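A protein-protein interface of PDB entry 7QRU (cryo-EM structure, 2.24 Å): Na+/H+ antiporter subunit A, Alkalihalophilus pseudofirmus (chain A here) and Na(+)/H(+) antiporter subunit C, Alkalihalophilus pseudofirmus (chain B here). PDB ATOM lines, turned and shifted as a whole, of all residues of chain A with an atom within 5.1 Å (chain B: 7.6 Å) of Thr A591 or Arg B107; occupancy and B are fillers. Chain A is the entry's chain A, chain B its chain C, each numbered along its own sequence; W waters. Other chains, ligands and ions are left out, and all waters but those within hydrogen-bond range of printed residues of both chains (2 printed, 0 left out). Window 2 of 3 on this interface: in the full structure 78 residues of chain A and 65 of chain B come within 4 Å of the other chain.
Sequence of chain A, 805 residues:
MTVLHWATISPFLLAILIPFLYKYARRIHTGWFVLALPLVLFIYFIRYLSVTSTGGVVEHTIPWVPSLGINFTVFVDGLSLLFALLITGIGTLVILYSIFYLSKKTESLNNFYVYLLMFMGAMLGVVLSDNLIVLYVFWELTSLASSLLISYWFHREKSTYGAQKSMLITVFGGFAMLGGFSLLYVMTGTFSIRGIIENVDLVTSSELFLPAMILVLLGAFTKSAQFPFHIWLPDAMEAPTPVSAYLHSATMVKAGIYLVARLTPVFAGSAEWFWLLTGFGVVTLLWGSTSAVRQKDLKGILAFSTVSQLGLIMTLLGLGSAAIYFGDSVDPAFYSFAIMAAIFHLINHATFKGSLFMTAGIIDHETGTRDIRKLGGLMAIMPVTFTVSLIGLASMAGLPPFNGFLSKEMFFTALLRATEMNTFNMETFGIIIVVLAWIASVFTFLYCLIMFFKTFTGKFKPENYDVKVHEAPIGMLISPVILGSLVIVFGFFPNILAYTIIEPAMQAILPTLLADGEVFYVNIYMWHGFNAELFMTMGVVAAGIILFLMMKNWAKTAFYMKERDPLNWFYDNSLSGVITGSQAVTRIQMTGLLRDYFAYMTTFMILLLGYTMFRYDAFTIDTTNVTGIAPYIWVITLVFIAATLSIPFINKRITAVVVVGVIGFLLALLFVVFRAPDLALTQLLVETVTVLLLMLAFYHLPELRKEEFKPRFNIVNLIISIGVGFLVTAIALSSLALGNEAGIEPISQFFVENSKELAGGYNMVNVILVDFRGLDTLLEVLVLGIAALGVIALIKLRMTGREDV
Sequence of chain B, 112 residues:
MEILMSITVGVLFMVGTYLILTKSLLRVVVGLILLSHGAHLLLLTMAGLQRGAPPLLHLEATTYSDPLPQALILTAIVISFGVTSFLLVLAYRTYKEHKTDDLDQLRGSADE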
ATOM      1  N   ARG A 587      -3.139 -16.875  10.467  1.00  0.00           N
ATOM      2  CA  ARG A 587      -3.147 -16.785  11.923  1.00  0.00           C
ATOM      3  C   ARG A 587      -2.441 -17.990  12.570  1.00  0.00           C
ATOM      4  O   ARG A 587      -1.745 -17.797  13.558  1.00  0.00           O
ATOM      5  CB  ARG A 587      -4.554 -16.486  12.404  1.00  0.00           C
ATOM      6  CG  ARG A 587      -4.981 -15.065  11.978  1.00  0.00           C
ATOM      7  CD  ARG A 587      -6.338 -14.473  12.428  1.00  0.00           C
ATOM      8  NE  ARG A 587      -7.553 -15.269  12.179  1.00  0.00           N
ATOM      9  CZ  ARG A 587      -7.869 -16.397  12.824  1.00  0.00           C
ATOM     10  NH1 ARG A 587      -7.113 -16.802  13.837  1.00  0.00           N
ATOM     11  NH2 ARG A 587      -8.900 -17.131  12.424  1.00  0.00           N
ATOM     12  N   ILE A 588      -2.477 -19.178  11.984  1.00  0.00           N
ATOM     13  CA  ILE A 588      -1.871 -20.302  12.642  1.00  0.00           C
ATOM     14  C   ILE A 588      -0.348 -20.172  12.510  1.00  0.00           C
ATOM     15  O   ILE A 588       0.403 -20.725  13.304  1.00  0.00           O
ATOM     16  CB  ILE A 588      -2.331 -21.712  12.164  1.00  0.00           C
ATOM     17  CG1 ILE A 588      -1.897 -21.961  10.769  1.00  0.00           C
ATOM     18  CG2 ILE A 588      -3.784 -21.983  12.250  1.00  0.00           C
ATOM     19  CD1 ILE A 588      -0.784 -22.962  10.742  1.00  0.00           C
ATOM     20  N   GLN A 589       0.149 -19.529  11.503  1.00  0.00           N
ATOM     21  CA  GLN A 589       1.576 -19.344  11.449  1.00  0.00           C
ATOM     22  C   GLN A 589       2.015 -18.109  12.269  1.00  0.00           C
ATOM     23  O   GLN A 589       2.962 -18.151  12.990  1.00  0.00           O
ATOM     24  CB  GLN A 589       1.947 -19.140  10.018  1.00  0.00           C
ATOM     25  CG  GLN A 589       1.533 -20.280   9.118  1.00  0.00           C
ATOM     26  CD  GLN A 589       1.787 -19.739   7.742  1.00  0.00           C
ATOM     27  OE1 GLN A 589       2.940 -19.537   7.346  1.00  0.00           O
ATOM     28  NE2 GLN A 589       0.707 -19.402   7.066  1.00  0.00           N
ATOM     29  N   MET A 590       1.354 -17.002  12.109  1.00  0.00           N
ATOM     30  CA  MET A 590       1.813 -15.776  12.633  1.00  0.00           C
ATOM     31  C   MET A 590       1.023 -15.501  13.891  1.00  0.00           C
ATOM     32  O   MET A 590       0.268 -14.563  13.931  1.00  0.00           O
ATOM     33  CB  MET A 590       1.605 -14.629  11.655  1.00  0.00           C
ATOM     34  CG  MET A 590       2.239 -14.919  10.324  1.00  0.00           C
ATOM     35  SD  MET A 590       4.039 -14.831  10.389  1.00  0.00           S
ATOM     36  CE  MET A 590       4.410 -13.303  11.267  1.00  0.00           C
ATOM     37  N   THR A 591       1.437 -16.183  14.941  1.00  0.00           N
ATOM     38  CA  THR A 591       0.787 -16.190  16.212  1.00  0.00           C
ATOM     39  C   THR A 591       1.269 -15.028  17.036  1.00  0.00           C
ATOM     40  O   THR A 591       0.575 -14.661  17.953  1.00  0.00           O
ATOM     41  CB  THR A 591       1.079 -17.514  16.896  1.00  0.00           C
ATOM     42  OG1 THR A 591       2.443 -17.556  17.309  1.00  0.00           O
ATOM     43  CG2 THR A 591       0.913 -18.653  15.932  1.00  0.00           C
ATOM     44  N   GLY A 592       2.398 -14.419  16.672  1.00  0.00           N
ATOM     45  CA  GLY A 592       2.918 -13.348  17.503  1.00  0.00           C
ATOM     46  C   GLY A 592       3.843 -13.879  18.602  1.00  0.00           C
ATOM     47  O   GLY A 592       4.459 -13.110  19.303  1.00  0.00           O
ATOM     48  N   LEU A 593       3.914 -15.195  18.749  1.00  0.00           N
ATOM     49  CA  LEU A 593       4.631 -15.753  19.864  1.00  0.00           C
ATOM     50  C   LEU A 593       6.026 -16.278  19.433  1.00  0.00           C
ATOM     51  O   LEU A 593       6.146 -17.119  18.556  1.00  0.00           O
ATOM     52  CB  LEU A 593       3.738 -16.804  20.467  1.00  0.00           C
ATOM     53  CG  LEU A 593       4.346 -17.324  21.756  1.00  0.00           C
ATOM     54  CD1 LEU A 593       4.230 -16.313  22.893  1.00  0.00           C
ATOM     55  CD2 LEU A 593       3.698 -18.635  22.145  1.00  0.00           C
ATOM     56  N   ASP A 596       6.624 -19.929  19.244  1.00  0.00           N
ATOM     57  CA  ASP A 596       6.088 -20.648  18.076  1.00  0.00           C
ATOM     58  C   ASP A 596       7.015 -20.472  16.903  1.00  0.00           C
ATOM     59  O   ASP A 596       7.275 -21.421  16.217  1.00  0.00           O
ATOM     60  CB  ASP A 596       4.737 -20.125  17.683  1.00  0.00           C
ATOM     61  CG  ASP A 596       3.683 -20.411  18.758  1.00  0.00           C
ATOM     62  OD1 ASP A 596       3.963 -21.266  19.642  1.00  0.00           O
ATOM     63  OD2 ASP A 596       2.545 -19.804  18.682  1.00  0.00           O
ATOM     64  N   TYR A 597       7.519 -19.233  16.668  1.00  0.00           N
ATOM     65  CA  TYR A 597       8.416 -19.096  15.540  1.00  0.00           C
ATOM     66  C   TYR A 597       9.662 -19.949  15.686  1.00  0.00           C
ATOM     67  O   TYR A 597      10.033 -20.646  14.711  1.00  0.00           O
ATOM     68  CB  TYR A 597       8.789 -17.658  15.293  1.00  0.00           C
ATOM     69  CG  TYR A 597       7.593 -16.765  15.206  1.00  0.00           C
ATOM     70  CD1 TYR A 597       6.398 -17.226  14.635  1.00  0.00           C
ATOM     71  CD2 TYR A 597       7.722 -15.421  15.526  1.00  0.00           C
ATOM     72  CE1 TYR A 597       5.307 -16.387  14.512  1.00  0.00           C
ATOM     73  CE2 TYR A 597       6.617 -14.609  15.456  1.00  0.00           C
ATOM     74  CZ  TYR A 597       5.410 -15.084  14.926  1.00  0.00           C
ATOM     75  OH  TYR A 597       4.326 -14.258  14.818  1.00  0.00           O
ATOM     76  N   TYR A 600       8.605 -23.701  15.120  1.00  0.00           N
ATOM     77  CA  TYR A 600       8.420 -24.058  13.714  1.00  0.00           C
ATOM     78  C   TYR A 600       9.746 -24.197  12.967  1.00  0.00           C
ATOM     79  O   TYR A 600      10.025 -25.177  12.301  1.00  0.00           O
ATOM     80  CB  TYR A 600       7.660 -23.009  12.943  1.00  0.00           C
ATOM     81  CG  TYR A 600       6.266 -22.761  13.400  1.00  0.00           C
ATOM     82  CD1 TYR A 600       5.531 -23.724  14.047  1.00  0.00           C
ATOM     83  CD2 TYR A 600       5.703 -21.511  13.220  1.00  0.00           C
ATOM     84  CE1 TYR A 600       4.247 -23.466  14.494  1.00  0.00           C
ATOM     85  CE2 TYR A 600       4.409 -21.241  13.639  1.00  0.00           C
ATOM     86  CZ  TYR A 600       3.675 -22.228  14.271  1.00  0.00           C
ATOM     87  OH  TYR A 600       2.406 -21.940  14.679  1.00  0.00           O
ATOM     88  N   THR B 100       6.221  -5.467  30.576  1.00  0.00           N
ATOM     89  CA  THR B 100       6.211  -6.934  30.715  1.00  0.00           C
ATOM     90  C   THR B 100       7.440  -7.552  30.106  1.00  0.00           C
ATOM     91  O   THR B 100       7.956  -6.998  29.140  1.00  0.00           O
ATOM     92  CB  THR B 100       4.939  -7.532  30.075  1.00  0.00           C
ATOM     93  OG1 THR B 100       5.025  -8.942  30.231  1.00  0.00           O
ATOM     94  CG2 THR B 100       4.720  -7.166  28.621  1.00  0.00           C
ATOM     95  N   ASP B 102       7.328 -11.040  29.825  1.00  0.00           N
ATOM     96  CA  ASP B 102       6.679 -12.219  29.291  1.00  0.00           C
ATOM     97  C   ASP B 102       6.394 -12.061  27.801  1.00  0.00           C
ATOM     98  O   ASP B 102       5.716 -11.124  27.372  1.00  0.00           O
ATOM     99  CB  ASP B 102       5.375 -12.413  30.022  1.00  0.00           C
ATOM    100  CG  ASP B 102       4.648 -13.674  29.652  1.00  0.00           C
ATOM    101  OD1 ASP B 102       5.256 -14.489  28.884  1.00  0.00           O
ATOM    102  OD2 ASP B 102       3.465 -13.830  30.159  1.00  0.00           O
ATOM    103  N   LEU B 103       6.944 -12.949  26.987  1.00  0.00           N
ATOM    104  CA  LEU B 103       6.754 -12.896  25.544  1.00  0.00           C
ATOM    105  C   LEU B 103       5.324 -13.230  25.101  1.00  0.00           C
ATOM    106  O   LEU B 103       4.885 -12.743  24.027  1.00  0.00           O
ATOM    107  CB  LEU B 103       7.764 -13.836  24.922  1.00  0.00           C
ATOM    108  CG  LEU B 103       9.176 -13.247  24.894  1.00  0.00           C
ATOM    109  CD1 LEU B 103      10.200 -14.386  24.852  1.00  0.00           C
ATOM    110  CD2 LEU B 103       9.348 -12.341  23.678  1.00  0.00           C
ATOM    111  N   ASP B 104       4.555 -13.949  25.945  1.00  0.00           N
ATOM    112  CA  ASP B 104       3.125 -14.143  25.697  1.00  0.00           C
ATOM    113  C   ASP B 104       2.353 -12.810  25.666  1.00  0.00           C
ATOM    114  O   ASP B 104       1.454 -12.630  24.830  1.00  0.00           O
ATOM    115  CB  ASP B 104       2.471 -15.053  26.720  1.00  0.00           C
ATOM    116  CG  ASP B 104       2.889 -16.494  26.589  1.00  0.00           C
ATOM    117  OD1 ASP B 104       4.071 -16.716  26.238  1.00  0.00           O
ATOM    118  OD2 ASP B 104       2.044 -17.380  26.854  1.00  0.00           O
ATOM    119  N   GLN B 105       2.783 -11.856  26.485  1.00  0.00           N
ATOM    120  CA  GLN B 105       2.148 -10.560  26.537  1.00  0.00           C
ATOM    121  C   GLN B 105       2.630  -9.670  25.412  1.00  0.00           C
ATOM    122  O   GLN B 105       2.064  -8.605  25.216  1.00  0.00           O
ATOM    123  CB  GLN B 105       2.438  -9.841  27.850  1.00  0.00           C
ATOM    124  CG  GLN B 105       2.222 -10.697  29.106  1.00  0.00           C
ATOM    125  CD  GLN B 105       0.808 -11.162  29.217  1.00  0.00           C
ATOM    126  OE1 GLN B 105      -0.121 -10.388  28.987  1.00  0.00           O
ATOM    127  NE2 GLN B 105       0.634 -12.425  29.599  1.00  0.00           N
ATOM    128  N   LEU B 106       3.686 -10.076  24.705  1.00  0.00           N
ATOM    129  CA  LEU B 106       4.230  -9.264  23.614  1.00  0.00           C
ATOM    130  C   LEU B 106       3.708  -9.759  22.273  1.00  0.00           C
ATOM    131  O   LEU B 106       4.328  -9.527  21.251  1.00  0.00           O
ATOM    132  CB  LEU B 106       5.768  -9.304  23.676  1.00  0.00           C
ATOM    133  CG  LEU B 106       6.315  -8.672  24.947  1.00  0.00           C
ATOM    134  CD1 LEU B 106       7.803  -8.838  25.079  1.00  0.00           C
ATOM    135  CD2 LEU B 106       5.982  -7.234  25.005  1.00  0.00           C
ATOM    136  N   ARG B 107       2.639 -10.551  22.252  1.00  0.00           N
ATOM    137  CA  ARG B 107       2.119 -11.088  20.995  1.00  0.00           C
ATOM    138  C   ARG B 107       1.616  -9.995  20.062  1.00  0.00           C
ATOM    139  O   ARG B 107       1.830 -10.091  18.853  1.00  0.00           O
ATOM    140  CB  ARG B 107       0.968 -12.052  21.229  1.00  0.00           C
ATOM    141  CG  ARG B 107       1.373 -13.440  21.668  1.00  0.00           C
ATOM    142  CD  ARG B 107       0.067 -14.171  21.916  1.00  0.00           C
ATOM    143  NE  ARG B 107       0.155 -15.579  22.255  1.00  0.00           N
ATOM    144  CZ  ARG B 107       0.229 -16.541  21.344  1.00  0.00           C
ATOM    145  NH1 ARG B 107      -0.082 -16.267  20.086  1.00  0.00           N
ATOM    146  NH2 ARG B 107       0.600 -17.768  21.689  1.00  0.00           N
ATOM    147  N   GLY B 108       0.972  -8.954  20.601  1.00  0.00           N
ATOM    148  CA  GLY B 108       0.358  -7.920  19.766  1.00  0.00           C
ATOM    149  C   GLY B 108      -1.041  -8.300  19.296  1.00  0.00           C
ATOM    150  O   GLY B 108      -1.578  -9.347  19.685  1.00  0.00           O
ATOM    151  N   SER B 109      -1.676  -7.416  18.495  1.00  0.00           N
ATOM    152  CA  SER B 109      -3.011  -7.660  17.922  1.00  0.00           C
ATOM    153  C   SER B 109      -2.991  -8.828  16.922  1.00  0.00           C
ATOM    154  O   SER B 109      -1.964  -9.071  16.272  1.00  0.00           O
ATOM    155  CB  SER B 109      -3.540  -6.409  17.285  1.00  0.00           C
ATOM    156  OG  SER B 109      -4.822  -6.638  16.710  1.00  0.00           O
ATOM    157  N   ALA B 110      -4.093  -9.601  16.854  1.00  0.00           N
ATOM    158  CA  ALA B 110      -4.171 -10.802  16.017  1.00  0.00           C
ATOM    159  C   ALA B 110      -4.693 -10.435  14.621  1.00  0.00           C
ATOM    160  O   ALA B 110      -5.655  -9.675  14.513  1.00  0.00           O
ATOM    161  CB  ALA B 110      -5.039 -11.858  16.686  1.00  0.00           C
ATOM    162  N   ASP B 111      -4.045 -10.950  13.556  1.00  0.00           N
ATOM    163  CA  ASP B 111      -4.269 -10.454  12.202  1.00  0.00           C
ATOM    164  C   ASP B 111      -4.053  -8.935  12.235  1.00  0.00           C
ATOM    165  O   ASP B 111      -5.004  -8.179  12.039  1.00  0.00           O
ATOM    166  CB  ASP B 111      -5.663 -10.884  11.695  1.00  0.00           C
ATOM    167  CG  ASP B 111      -5.806 -11.261  10.217  1.00  0.00           C
ATOM    168  OD1 ASP B 111      -5.486 -10.415   9.342  1.00  0.00           O
ATOM    169  OD2 ASP B 111      -6.286 -12.395   9.946  1.00  0.00           O
ATOM    170  N   GLU B 112      -2.804  -8.491  12.500  1.00  0.00           N
ATOM    171  CA  GLU B 112      -2.545  -7.169  13.088  1.00  0.00           C
ATOM    172  C   GLU B 112      -3.470  -6.100  12.455  1.00  0.00           C
ATOM    173  O   GLU B 112      -3.045  -5.498  11.433  1.00  0.00           O
ATOM    174  CB  GLU B 112      -1.050  -6.790  13.006  1.00  0.00           C
ATOM    175  CG  GLU B 112      -0.140  -7.510  13.991  1.00  0.00           C
ATOM    176  CD  GLU B 112       0.361  -6.898  15.312  1.00  0.00           C
ATOM    177  OE1 GLU B 112       1.209  -7.588  15.941  1.00  0.00           O
ATOM    178  OE2 GLU B 112      -0.057  -5.773  15.759  1.00  0.00           O
ATOM    179  OXT GLU B 112      -4.597  -5.868  13.021  1.00  0.00           O
HETATM  180  O   HOH W   1       6.040 -13.030  21.491  1.00  0.00           O
HETATM  181  O   HOH W   2       0.397 -20.507  19.805  1.00  0.00           O
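The side-chain carboxylate (OD2) of Asp B111 lies within salt-bridge range of the guanidinium group (NE) of Arg A587 (3.9 Å).
O of Thr A591 sits at hydrogen-bond distance from NH1 of Arg B107, 2.7 Å away.
OG1 of Thr A591 lies within hydrogen-bond range of N of Leu A593 (3.1 Å).
OD1 of Asp B102 lies within hydrogen-bond range of N of Asp B104, at 3.1 Å.
OH of Tyr A597 is in hydrogen-bond range of N of Thr A591, at 3.5 Å.
The side-chain hydroxyl of Thr A591 sits at hydrogen-bond distance from the side-chain carboxylate of Asp A596, 2.6 Å away.
The backbone NH (N) of Gly A592 lies within hydrogen-bond range of the side-chain hydroxyl (OH) of Tyr A597 (2.7 Å).
Among the printed residues, pairs that only touch across the chains: Gly A592 with Arg B107 (3.5 Å), Leu A593 with Leu B103 (3.8 Å), Leu A593 with Asp B104 (3.4 Å) and Leu A593 with Arg B107 (3.2 Å).
Thr A591 touches just one residue of chain B: Arg B107 (2.7 Å).
Of the printed residues of chain A, Arg B107 touches Thr A591 (2.7 Å), Gly A592 (3.5 Å) and Leu A593 (3.2 Å).
Of chain B, only Arg B107 comes within 4 Å of Gly A592.
Printed residues of chain B within 4 Å of Arg A587: Asp B111.
Printed residues of chain A within 4 Å of Asp B111: Arg A587 (3.2 Å).
Of the printed residues of chain A, Leu B103 touches Leu A593 (3.8 Å).
Printed residues of chain B within 4 Å of Leu A593: Leu B103 (3.8 Å), Asp B104 (3.4 Å) and Arg B107 (3.2 Å).
Of the printed residues of chain A, Asp B104 touches Leu A593 (3.4 Å).
Ser B109 touches none of the printed residues of chain A.
The nearest residue of chain B that does not touch Thr A591 is Gly B108 (6.0 Å).
The nearest residue of chain A that does not touch Arg B107 is Asp A596 (4.1 Å).
The nearest printed residue of chain A that does not touch Asp B111 is Met A590 (5.6 Å).
Of the 10 printed residues of chain A, 4 touch a printed residue of chain B.
Among the printed residues, Asp or Glu carboxylates within 4 Å of a Lys or Arg side-chain nitrogen of the other chain: Arg A587 with Asp B111 (3.9 Å).
Water W2 lies within hydrogen-bond range of the side-chain carboxylate (OD2) of Asp A596 (2.5 Å) and the guanidinium group (NH2) of Arg B107 (3.3 Å).
Water W1 lies within hydrogen-bond range of O of Gly A592 (2.7 Å) and O of Leu B103 (2.8 Å).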
